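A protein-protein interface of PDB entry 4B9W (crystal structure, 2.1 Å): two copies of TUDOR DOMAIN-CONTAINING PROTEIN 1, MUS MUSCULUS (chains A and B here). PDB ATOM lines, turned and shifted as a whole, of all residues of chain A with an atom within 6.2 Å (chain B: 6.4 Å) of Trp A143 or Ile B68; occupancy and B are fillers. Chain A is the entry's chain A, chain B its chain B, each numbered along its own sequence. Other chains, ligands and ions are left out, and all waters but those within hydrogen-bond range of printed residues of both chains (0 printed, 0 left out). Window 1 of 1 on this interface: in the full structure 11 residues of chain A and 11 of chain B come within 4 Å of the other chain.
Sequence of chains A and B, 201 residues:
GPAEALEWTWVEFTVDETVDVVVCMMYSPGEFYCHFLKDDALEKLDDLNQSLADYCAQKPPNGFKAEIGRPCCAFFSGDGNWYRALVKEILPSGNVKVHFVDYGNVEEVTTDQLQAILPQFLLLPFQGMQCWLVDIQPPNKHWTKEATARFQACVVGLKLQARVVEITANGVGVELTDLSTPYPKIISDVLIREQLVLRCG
No position is printed for both chains.
Ile A136 touches none of the printed residues of chain B.
Of the printed residues of chain B, Trp A143 touches Ile B68 (3.5 Å).
Printed residues of chain B within 4 Å of Thr A144: Glu B67.
Printed residues of chain B within 4 Å of Lys A145: Ala B66 (2.7 Å), Glu B67 (3.0 Å) and Ile B90 (3.3 Å).
Ile B68 touches two residues of chain A.
The nearest residue of chain A that does not touch Ile B68 is Lys A145 (4.8 Å).
Of the 9 printed residues of chain B, 5 touch a printed residue of chain A.
Printed residues of chain B that touch a printed residue of chain A: Ala B66, Glu B67, Ile B68, Gly B69 and Ile B90.
Printed residues of chain A that touch a printed residue of chain B: His A142, Trp A143, Thr A144 and Lys A145.
Hydrophobic or aromatic side chains of chain A that line the printed part of chain B: His A142.
Among the printed residues, no Asp or Glu carboxylate lies within 4 Å of a Lys or Arg side-chain nitrogen of the other chain.
Among the printed residues, pairs that only touch across the chains: His A142 with Ile B68 (3.6 Å), His A142 with Gly B69 (3.5 Å), Trp A143 with Ile B68 (3.5 Å), Thr A144 with Glu B67 (3.5 Å) and Lys A145 with Ile B90 (3.3 Å).
The side-chain hydroxyl of Thr A144 lies within hydrogen-bond range of the backbone NH of Ala A147 (3.0 Å).
A ring nitrogen (NE2) of His A142 sits at hydrogen-bond distance from the side-chain amino group of Lys A141.
O of Val B87 is in hydrogen-bond range of N of Gly B69 (2.8 Å).
The side-chain hydroxyl (OG1) of Thr A148 is in hydrogen-bond range of the backbone carbonyl oxygen (O) of Thr A144, at 3.2 Å.
The side-chain amino group (NZ) of Lys A145 sits at hydrogen-bond distance from the backbone carbonyl oxygen (O) of Ala B66, at 2.7 Å.
N of Lys A145 is in hydrogen-bond range of OE2 of Glu B67, at 3.0 Å.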
ATOM      1  N   TYR A  27       0.258   4.072   7.318  1.00  0.00           N
ATOM      2  CA  TYR A  27      -0.702   5.092   6.957  1.00  0.00           C
ATOM      3  C   TYR A  27      -0.963   6.023   8.116  1.00  0.00           C
ATOM      4  O   TYR A  27      -1.121   7.221   7.899  1.00  0.00           O
ATOM      5  CB  TYR A  27      -2.019   4.465   6.509  1.00  0.00           C
ATOM      6  CG  TYR A  27      -1.930   3.630   5.278  1.00  0.00           C
ATOM      7  CD1 TYR A  27      -2.026   4.205   4.020  1.00  0.00           C
ATOM      8  CD2 TYR A  27      -1.746   2.251   5.360  1.00  0.00           C
ATOM      9  CE1 TYR A  27      -1.961   3.430   2.876  1.00  0.00           C
ATOM     10  CE2 TYR A  27      -1.670   1.477   4.223  1.00  0.00           C
ATOM     11  CZ  TYR A  27      -1.784   2.067   2.986  1.00  0.00           C
ATOM     12  OH  TYR A  27      -1.705   1.284   1.866  1.00  0.00           O
ATOM     13  N   SER A  28      -1.030   5.469   9.336  1.00  0.00           N
ATOM     14  CA  SER A  28      -1.265   6.235  10.582  1.00  0.00           C
ATOM     15  C   SER A  28      -0.974   5.385  11.812  1.00  0.00           C
ATOM     16  O   SER A  28      -0.665   4.211  11.687  1.00  0.00           O
ATOM     17  CB  SER A  28      -2.725   6.752  10.682  1.00  0.00           C
ATOM     18  OG  SER A  28      -3.660   5.723  10.944  1.00  0.00           O
ATOM     19  N   PRO A  29      -1.111   5.965  13.014  1.00  0.00           N
ATOM     20  CA  PRO A  29      -1.117   5.140  14.221  1.00  0.00           C
ATOM     21  C   PRO A  29      -2.300   4.206  14.335  1.00  0.00           C
ATOM     22  O   PRO A  29      -2.249   3.290  15.158  1.00  0.00           O
ATOM     23  CB  PRO A  29      -1.155   6.176  15.353  1.00  0.00           C
ATOM     24  CG  PRO A  29      -0.495   7.366  14.780  1.00  0.00           C
ATOM     25  CD  PRO A  29      -0.988   7.393  13.355  1.00  0.00           C
ATOM     26  N   GLY A  30      -3.355   4.427  13.545  1.00  0.00           N
ATOM     27  CA  GLY A  30      -4.534   3.579  13.560  1.00  0.00           C
ATOM     28  C   GLY A  30      -4.566   2.558  12.432  1.00  0.00           C
ATOM     29  O   GLY A  30      -5.503   1.748  12.322  1.00  0.00           O
ATOM     30  N   GLU A  31      -3.528   2.599  11.604  1.00  0.00           N
ATOM     31  CA  GLU A  31      -3.477   1.803  10.405  1.00  0.00           C
ATOM     32  C   GLU A  31      -2.050   1.647   9.883  1.00  0.00           C
ATOM     33  O   GLU A  31      -1.556   2.464   9.093  1.00  0.00           O
ATOM     34  CB  GLU A  31      -4.351   2.469   9.357  1.00  0.00           C
ATOM     35  CG  GLU A  31      -4.470   1.709   8.056  1.00  0.00           C
ATOM     36  CD  GLU A  31      -5.266   2.492   7.018  1.00  0.00           C
ATOM     37  OE1 GLU A  31      -5.385   3.746   7.118  1.00  0.00           O
ATOM     38  OE2 GLU A  31      -5.753   1.857   6.084  1.00  0.00           O
ATOM     39  N   LEU A 133      -2.185   0.984  17.020  1.00  0.00           N
ATOM     40  CA  LEU A 133      -1.686   1.083  18.389  1.00  0.00           C
ATOM     41  C   LEU A 133      -2.885   1.144  19.325  1.00  0.00           C
ATOM     42  O   LEU A 133      -3.865   1.794  19.024  1.00  0.00           O
ATOM     43  CB  LEU A 133      -0.829   2.339  18.592  1.00  0.00           C
ATOM     44  CG  LEU A 133       0.529   2.402  17.870  1.00  0.00           C
ATOM     45  CD1 LEU A 133       1.230   3.703  18.235  1.00  0.00           C
ATOM     46  CD2 LEU A 133       1.396   1.213  18.211  1.00  0.00           C
ATOM     47  N   ILE A 136      -4.817   4.826  22.299  1.00  0.00           N
ATOM     48  CA  ILE A 136      -4.733   6.208  21.784  1.00  0.00           C
ATOM     49  C   ILE A 136      -5.810   6.542  20.739  1.00  0.00           C
ATOM     50  O   ILE A 136      -6.437   5.666  20.171  1.00  0.00           O
ATOM     51  CB  ILE A 136      -3.354   6.498  21.167  1.00  0.00           C
ATOM     52  CG1 ILE A 136      -3.076   5.529  19.998  1.00  0.00           C
ATOM     53  CG2 ILE A 136      -2.260   6.418  22.228  1.00  0.00           C
ATOM     54  CD1 ILE A 136      -2.065   6.046  19.010  1.00  0.00           C
ATOM     55  N   GLN A 137      -6.005   7.832  20.505  1.00  0.00           N
ATOM     56  CA  GLN A 137      -6.988   8.345  19.548  1.00  0.00           C
ATOM     57  C   GLN A 137      -6.510   9.727  19.055  1.00  0.00           C
ATOM     58  O   GLN A 137      -5.744  10.396  19.751  1.00  0.00           O
ATOM     59  CB  GLN A 137      -8.368   8.464  20.228  1.00  0.00           C
ATOM     60  CG  GLN A 137      -8.408   9.449  21.409  1.00  0.00           C
ATOM     61  CD  GLN A 137      -9.764   9.490  22.092  1.00  0.00           C
ATOM     62  OE1 GLN A 137     -10.798   9.443  21.431  1.00  0.00           O
ATOM     63  NE2 GLN A 137      -9.766   9.564  23.425  1.00  0.00           N
ATOM     64  N   PRO A 138      -6.941  10.155  17.854  1.00  0.00           N
ATOM     65  CA  PRO A 138      -6.550  11.493  17.372  1.00  0.00           C
ATOM     66  C   PRO A 138      -7.124  12.612  18.242  1.00  0.00           C
ATOM     67  O   PRO A 138      -8.198  12.447  18.796  1.00  0.00           O
ATOM     68  CB  PRO A 138      -7.152  11.561  15.960  1.00  0.00           C
ATOM     69  CG  PRO A 138      -8.111  10.416  15.852  1.00  0.00           C
ATOM     70  CD  PRO A 138      -7.701   9.385  16.848  1.00  0.00           C
ATOM     71  N   PRO A 139      -6.396  13.728  18.402  1.00  0.00           N
ATOM     72  CA  PRO A 139      -6.930  14.842  19.213  1.00  0.00           C
ATOM     73  C   PRO A 139      -8.277  15.348  18.713  1.00  0.00           C
ATOM     74  O   PRO A 139      -9.180  15.567  19.510  1.00  0.00           O
ATOM     75  CB  PRO A 139      -5.861  15.927  19.078  1.00  0.00           C
ATOM     76  CG  PRO A 139      -4.602  15.184  18.787  1.00  0.00           C
ATOM     77  CD  PRO A 139      -4.997  13.961  18.001  1.00  0.00           C
ATOM     78  N   LYS A 141     -10.552  14.444  14.925  1.00  0.00           N
ATOM     79  CA  LYS A 141     -11.138  13.201  14.403  1.00  0.00           C
ATOM     80  C   LYS A 141     -10.246  12.486  13.388  1.00  0.00           C
ATOM     81  O   LYS A 141     -10.634  11.477  12.820  1.00  0.00           O
ATOM     82  CB  LYS A 141     -12.529  13.472  13.805  1.00  0.00           C
ATOM     83  CG  LYS A 141     -12.747  14.907  13.362  1.00  0.00           C
ATOM     84  CD  LYS A 141     -14.110  15.104  12.708  1.00  0.00           C
ATOM     85  CE  LYS A 141     -14.183  16.474  12.041  1.00  0.00           C
ATOM     86  NZ  LYS A 141     -13.097  16.621  11.027  1.00  0.00           N
ATOM     87  N   HIS A 142      -9.048  13.002  13.170  1.00  0.00           N
ATOM     88  CA  HIS A 142      -8.210  12.519  12.090  1.00  0.00           C
ATOM     89  C   HIS A 142      -6.811  12.516  12.574  1.00  0.00           C
ATOM     90  O   HIS A 142      -6.399  13.428  13.274  1.00  0.00           O
ATOM     91  CB  HIS A 142      -8.323  13.439  10.869  1.00  0.00           C
ATOM     92  CG  HIS A 142      -9.703  13.473  10.242  1.00  0.00           C
ATOM     93  ND1 HIS A 142     -10.204  12.439   9.532  1.00  0.00           N
ATOM     94  CD2 HIS A 142     -10.684  14.468  10.238  1.00  0.00           C
ATOM     95  CE1 HIS A 142     -11.441  12.753   9.092  1.00  0.00           C
ATOM     96  NE2 HIS A 142     -11.736  13.994   9.524  1.00  0.00           N
ATOM     97  N   TRP A 143      -6.077  11.474  12.207  1.00  0.00           N
ATOM     98  CA  TRP A 143      -4.641  11.416  12.459  1.00  0.00           C
ATOM     99  C   TRP A 143      -3.914  12.491  11.687  1.00  0.00           C
ATOM    100  O   TRP A 143      -4.014  12.548  10.459  1.00  0.00           O
ATOM    101  CB  TRP A 143      -4.101  10.049  12.052  1.00  0.00           C
ATOM    102  CG  TRP A 143      -4.736   8.910  12.793  1.00  0.00           C
ATOM    103  CD1 TRP A 143      -5.614   7.956  12.288  1.00  0.00           C
ATOM    104  CD2 TRP A 143      -4.568   8.560  14.213  1.00  0.00           C
ATOM    105  NE1 TRP A 143      -5.978   7.063  13.263  1.00  0.00           N
ATOM    106  CE2 TRP A 143      -5.381   7.364  14.437  1.00  0.00           C
ATOM    107  CE3 TRP A 143      -3.848   9.091  15.273  1.00  0.00           C
ATOM    108  CZ2 TRP A 143      -5.456   6.751  15.683  1.00  0.00           C
ATOM    109  CZ3 TRP A 143      -3.932   8.463  16.511  1.00  0.00           C
ATOM    110  CH2 TRP A 143      -4.719   7.322  16.710  1.00  0.00           C
ATOM    111  N   THR A 144      -3.186  13.358  12.382  1.00  0.00           N
ATOM    112  CA  THR A 144      -2.408  14.409  11.717  1.00  0.00           C
ATOM    113  C   THR A 144      -1.168  13.820  11.031  1.00  0.00           C
ATOM    114  O   THR A 144      -0.700  12.756  11.436  1.00  0.00           O
ATOM    115  CB  THR A 144      -1.953  15.484  12.720  1.00  0.00           C
ATOM    116  OG1 THR A 144      -1.163  14.874  13.754  1.00  0.00           O
ATOM    117  CG2 THR A 144      -3.165  16.206  13.333  1.00  0.00           C
ATOM    118  N   LYS A 145      -0.673  14.497   9.982  1.00  0.00           N
ATOM    119  CA  LYS A 145       0.627  14.187   9.360  1.00  0.00           C
ATOM    120  C   LYS A 145       1.746  14.156  10.397  1.00  0.00           C
ATOM    121  O   LYS A 145       2.614  13.285  10.370  1.00  0.00           O
ATOM    122  CB  LYS A 145       1.014  15.251   8.328  1.00  0.00           C
ATOM    123  CG  LYS A 145       0.269  15.219   7.020  1.00  0.00           C
ATOM    124  CD  LYS A 145       0.856  16.234   6.038  1.00  0.00           C
ATOM    125  CE  LYS A 145       0.486  17.671   6.375  1.00  0.00           C
ATOM    126  NZ  LYS A 145       0.874  18.606   5.288  1.00  0.00           N
ATOM    127  N   ALA A 147       1.498  13.575  13.715  1.00  0.00           N
ATOM    128  CA  ALA A 147       1.378  12.360  14.548  1.00  0.00           C
ATOM    129  C   ALA A 147       1.882  11.150  13.762  1.00  0.00           C
ATOM    130  O   ALA A 147       2.621  10.298  14.279  1.00  0.00           O
ATOM    131  CB  ALA A 147      -0.050  12.150  15.012  1.00  0.00           C
ATOM    132  N   THR A 148       1.529  11.093  12.487  1.00  0.00           N
ATOM    133  CA  THR A 148       1.947   9.959  11.655  1.00  0.00           C
ATOM    134  C   THR A 148       3.461   9.964  11.382  1.00  0.00           C
ATOM    135  O   THR A 148       4.119   8.924  11.498  1.00  0.00           O
ATOM    136  CB  THR A 148       1.091   9.878  10.371  1.00  0.00           C
ATOM    137  OG1 THR A 148      -0.285   9.677  10.744  1.00  0.00           O
ATOM    138  CG2 THR A 148       1.543   8.729   9.491  1.00  0.00           C
ATOM    139  N   LEU A 191       4.041   9.283  21.628  1.00  0.00           N
ATOM    140  CA  LEU A 191       2.984  10.069  20.972  1.00  0.00           C
ATOM    141  C   LEU A 191       2.070  10.821  21.954  1.00  0.00           C
ATOM    142  O   LEU A 191       1.594  11.921  21.649  1.00  0.00           O
ATOM    143  CB  LEU A 191       2.134   9.169  20.066  1.00  0.00           C
ATOM    144  CG  LEU A 191       2.836   8.442  18.903  1.00  0.00           C
ATOM    145  CD1 LEU A 191       1.805   7.775  17.990  1.00  0.00           C
ATOM    146  CD2 LEU A 191       3.737   9.364  18.099  1.00  0.00           C
ATOM    147  N   LEU A 196       0.740  14.616  20.514  1.00  0.00           N
ATOM    148  CA  LEU A 196       0.363  14.333  19.140  1.00  0.00           C
ATOM    149  C   LEU A 196      -0.880  13.450  19.055  1.00  0.00           C
ATOM    150  O   LEU A 196      -1.545  13.406  18.012  1.00  0.00           O
ATOM    151  CB  LEU A 196       1.505  13.652  18.412  1.00  0.00           C
ATOM    152  CG  LEU A 196       2.822  14.413  18.423  1.00  0.00           C
ATOM    153  CD1 LEU A 196       3.872  13.619  17.678  1.00  0.00           C
ATOM    154  CD2 LEU A 196       2.647  15.807  17.816  1.00  0.00           C
ATOM    155  N   VAL A 197      -1.183  12.739  20.141  1.00  0.00           N
ATOM    156  CA  VAL A 197      -2.382  11.887  20.209  1.00  0.00           C
ATOM    157  C   VAL A 197      -2.942  11.917  21.632  1.00  0.00           C
ATOM    158  O   VAL A 197      -2.280  12.365  22.560  1.00  0.00           O
ATOM    159  CB  VAL A 197      -2.100  10.435  19.775  1.00  0.00           C
ATOM    160  CG1 VAL A 197      -1.386  10.383  18.428  1.00  0.00           C
ATOM    161  CG2 VAL A 197      -1.294   9.708  20.834  1.00  0.00           C
ATOM    162  N   LEU A 198      -4.169  11.462  21.794  1.00  0.00           N
ATOM    163  CA  LEU A 198      -4.830  11.501  23.087  1.00  0.00           C
ATOM    164  C   LEU A 198      -4.984  10.095  23.609  1.00  0.00           C
ATOM    165  O   LEU A 198      -5.152   9.175  22.818  1.00  0.00           O
ATOM    166  CB  LEU A 198      -6.213  12.151  22.987  1.00  0.00           C
ATOM    167  CG  LEU A 198      -6.285  13.674  22.976  1.00  0.00           C
ATOM    168  CD1 LEU A 198      -7.737  14.068  23.166  1.00  0.00           C
ATOM    169  CD2 LEU A 198      -5.393  14.276  24.058  1.00  0.00           C
ATOM    170  N   ALA B  66      -2.417  21.418   2.882  1.00  0.00           N
ATOM    171  CA  ALA B  66      -3.114  20.128   3.070  1.00  0.00           C
ATOM    172  C   ALA B  66      -2.844  19.475   4.429  1.00  0.00           C
ATOM    173  O   ALA B  66      -1.702  19.343   4.863  1.00  0.00           O
ATOM    174  CB  ALA B  66      -2.795  19.152   1.929  1.00  0.00           C
ATOM    175  N   GLU B  67      -3.931  19.113   5.103  1.00  0.00           N
ATOM    176  CA  GLU B  67      -3.912  18.327   6.311  1.00  0.00           C
ATOM    177  C   GLU B  67      -5.064  17.318   6.202  1.00  0.00           C
ATOM    178  O   GLU B  67      -6.122  17.634   5.661  1.00  0.00           O
ATOM    179  CB  GLU B  67      -4.066  19.222   7.545  1.00  0.00           C
ATOM    180  CG  GLU B  67      -3.991  18.473   8.873  1.00  0.00           C
ATOM    181  CD  GLU B  67      -2.673  17.712   9.084  1.00  0.00           C
ATOM    182  OE1 GLU B  67      -1.667  18.360   9.453  1.00  0.00           O
ATOM    183  OE2 GLU B  67      -2.646  16.478   8.897  1.00  0.00           O
ATOM    184  N   ILE B  68      -4.834  16.105   6.705  1.00  0.00           N
ATOM    185  CA  ILE B  68      -5.836  15.036   6.688  1.00  0.00           C
ATOM    186  C   ILE B  68      -7.114  15.474   7.382  1.00  0.00           C
ATOM    187  O   ILE B  68      -7.078  15.941   8.526  1.00  0.00           O
ATOM    188  CB  ILE B  68      -5.319  13.767   7.395  1.00  0.00           C
ATOM    189  CG1 ILE B  68      -4.082  13.218   6.678  1.00  0.00           C
ATOM    190  CG2 ILE B  68      -6.412  12.710   7.465  1.00  0.00           C
ATOM    191  CD1 ILE B  68      -4.199  13.180   5.165  1.00  0.00           C
ATOM    192  N   GLY B  69      -8.231  15.329   6.669  1.00  0.00           N
ATOM    193  CA  GLY B  69      -9.546  15.703   7.162  1.00  0.00           C
ATOM    194  C   GLY B  69      -9.892  17.176   7.071  1.00  0.00           C
ATOM    195  O   GLY B  69     -10.936  17.593   7.532  1.00  0.00           O
ATOM    196  N   ARG B  70      -9.026  17.965   6.454  1.00  0.00           N
ATOM    197  CA  ARG B  70      -9.263  19.399   6.303  1.00  0.00           C
ATOM    198  C   ARG B  70     -10.124  19.696   5.062  1.00  0.00           C
ATOM    199  O   ARG B  70      -9.918  19.088   3.999  1.00  0.00           O
ATOM    200  CB  ARG B  70      -7.938  20.172   6.206  1.00  0.00           C
ATOM    201  CG  ARG B  70      -8.128  21.687   6.309  1.00  0.00           C
ATOM    202  CD  ARG B  70      -6.845  22.469   6.067  1.00  0.00           C
ATOM    203  NE  ARG B  70      -5.820  22.173   7.073  1.00  0.00           N
ATOM    204  CZ  ARG B  70      -5.576  22.895   8.167  1.00  0.00           C
ATOM    205  NH1 ARG B  70      -6.266  24.002   8.442  1.00  0.00           N
ATOM    206  NH2 ARG B  70      -4.619  22.503   9.000  1.00  0.00           N
ATOM    207  N   VAL B  87      -9.659  16.569   2.509  1.00  0.00           N
ATOM    208  CA  VAL B  87      -8.422  15.843   2.242  1.00  0.00           C
ATOM    209  C   VAL B  87      -8.478  14.462   2.874  1.00  0.00           C
ATOM    210  O   VAL B  87      -8.623  14.334   4.092  1.00  0.00           O
ATOM    211  CB  VAL B  87      -7.183  16.589   2.797  1.00  0.00           C
ATOM    212  CG1 VAL B  87      -5.915  15.777   2.556  1.00  0.00           C
ATOM    213  CG2 VAL B  87      -7.046  17.959   2.155  1.00  0.00           C
ATOM    214  N   LYS B  88      -8.312  13.430   2.058  1.00  0.00           N
ATOM    215  CA  LYS B  88      -8.400  12.046   2.537  1.00  0.00           C
ATOM    216  C   LYS B  88      -7.009  11.447   2.685  1.00  0.00           C
ATOM    217  O   LYS B  88      -6.681  10.875   3.728  1.00  0.00           O
ATOM    218  CB  LYS B  88      -9.303  11.209   1.618  1.00  0.00           C
ATOM    219  CG  LYS B  88      -9.389   9.722   1.971  1.00  0.00           C
ATOM    220  CD  LYS B  88     -10.745   9.116   1.623  1.00  0.00           C
ATOM    221  CE  LYS B  88     -11.716   9.184   2.800  1.00  0.00           C
ATOM    222  NZ  LYS B  88     -11.897   7.843   3.425  1.00  0.00           N
ATOM    223  N   GLU B  89      -6.177  11.603   1.663  1.00  0.00           N
ATOM    224  CA  GLU B  89      -4.806  11.092   1.723  1.00  0.00           C
ATOM    225  C   GLU B  89      -3.803  12.089   1.184  1.00  0.00           C
ATOM    226  O   GLU B  89      -4.143  12.913   0.333  1.00  0.00           O
ATOM    227  CB  GLU B  89      -4.675   9.786   0.933  1.00  0.00           C
ATOM    228  CG  GLU B  89      -5.876   8.851   1.043  1.00  0.00           C
ATOM    229  CD  GLU B  89      -5.581   7.479   0.474  1.00  0.00           C
ATOM    230  OE1 GLU B  89      -4.605   7.350  -0.280  1.00  0.00           O
ATOM    231  OE2 GLU B  89      -6.312   6.523   0.796  1.00  0.00           O
ATOM    232  N   ILE B  90      -2.572  12.008   1.687  1.00  0.00           N
ATOM    233  CA  ILE B  90      -1.444  12.750   1.124  1.00  0.00           C
ATOM    234  C   ILE B  90      -0.361  11.747   0.703  1.00  0.00           C
ATOM    235  O   ILE B  90       0.128  10.947   1.514  1.00  0.00           O
ATOM    236  CB  ILE B  90      -0.847  13.768   2.098  1.00  0.00           C
ATOM    237  CG1 ILE B  90      -1.904  14.794   2.545  1.00  0.00           C
ATOM    238  CG2 ILE B  90       0.355  14.484   1.463  1.00  0.00           C
ATOM    239  CD1 ILE B  90      -1.420  15.634   3.703  1.00  0.00           C
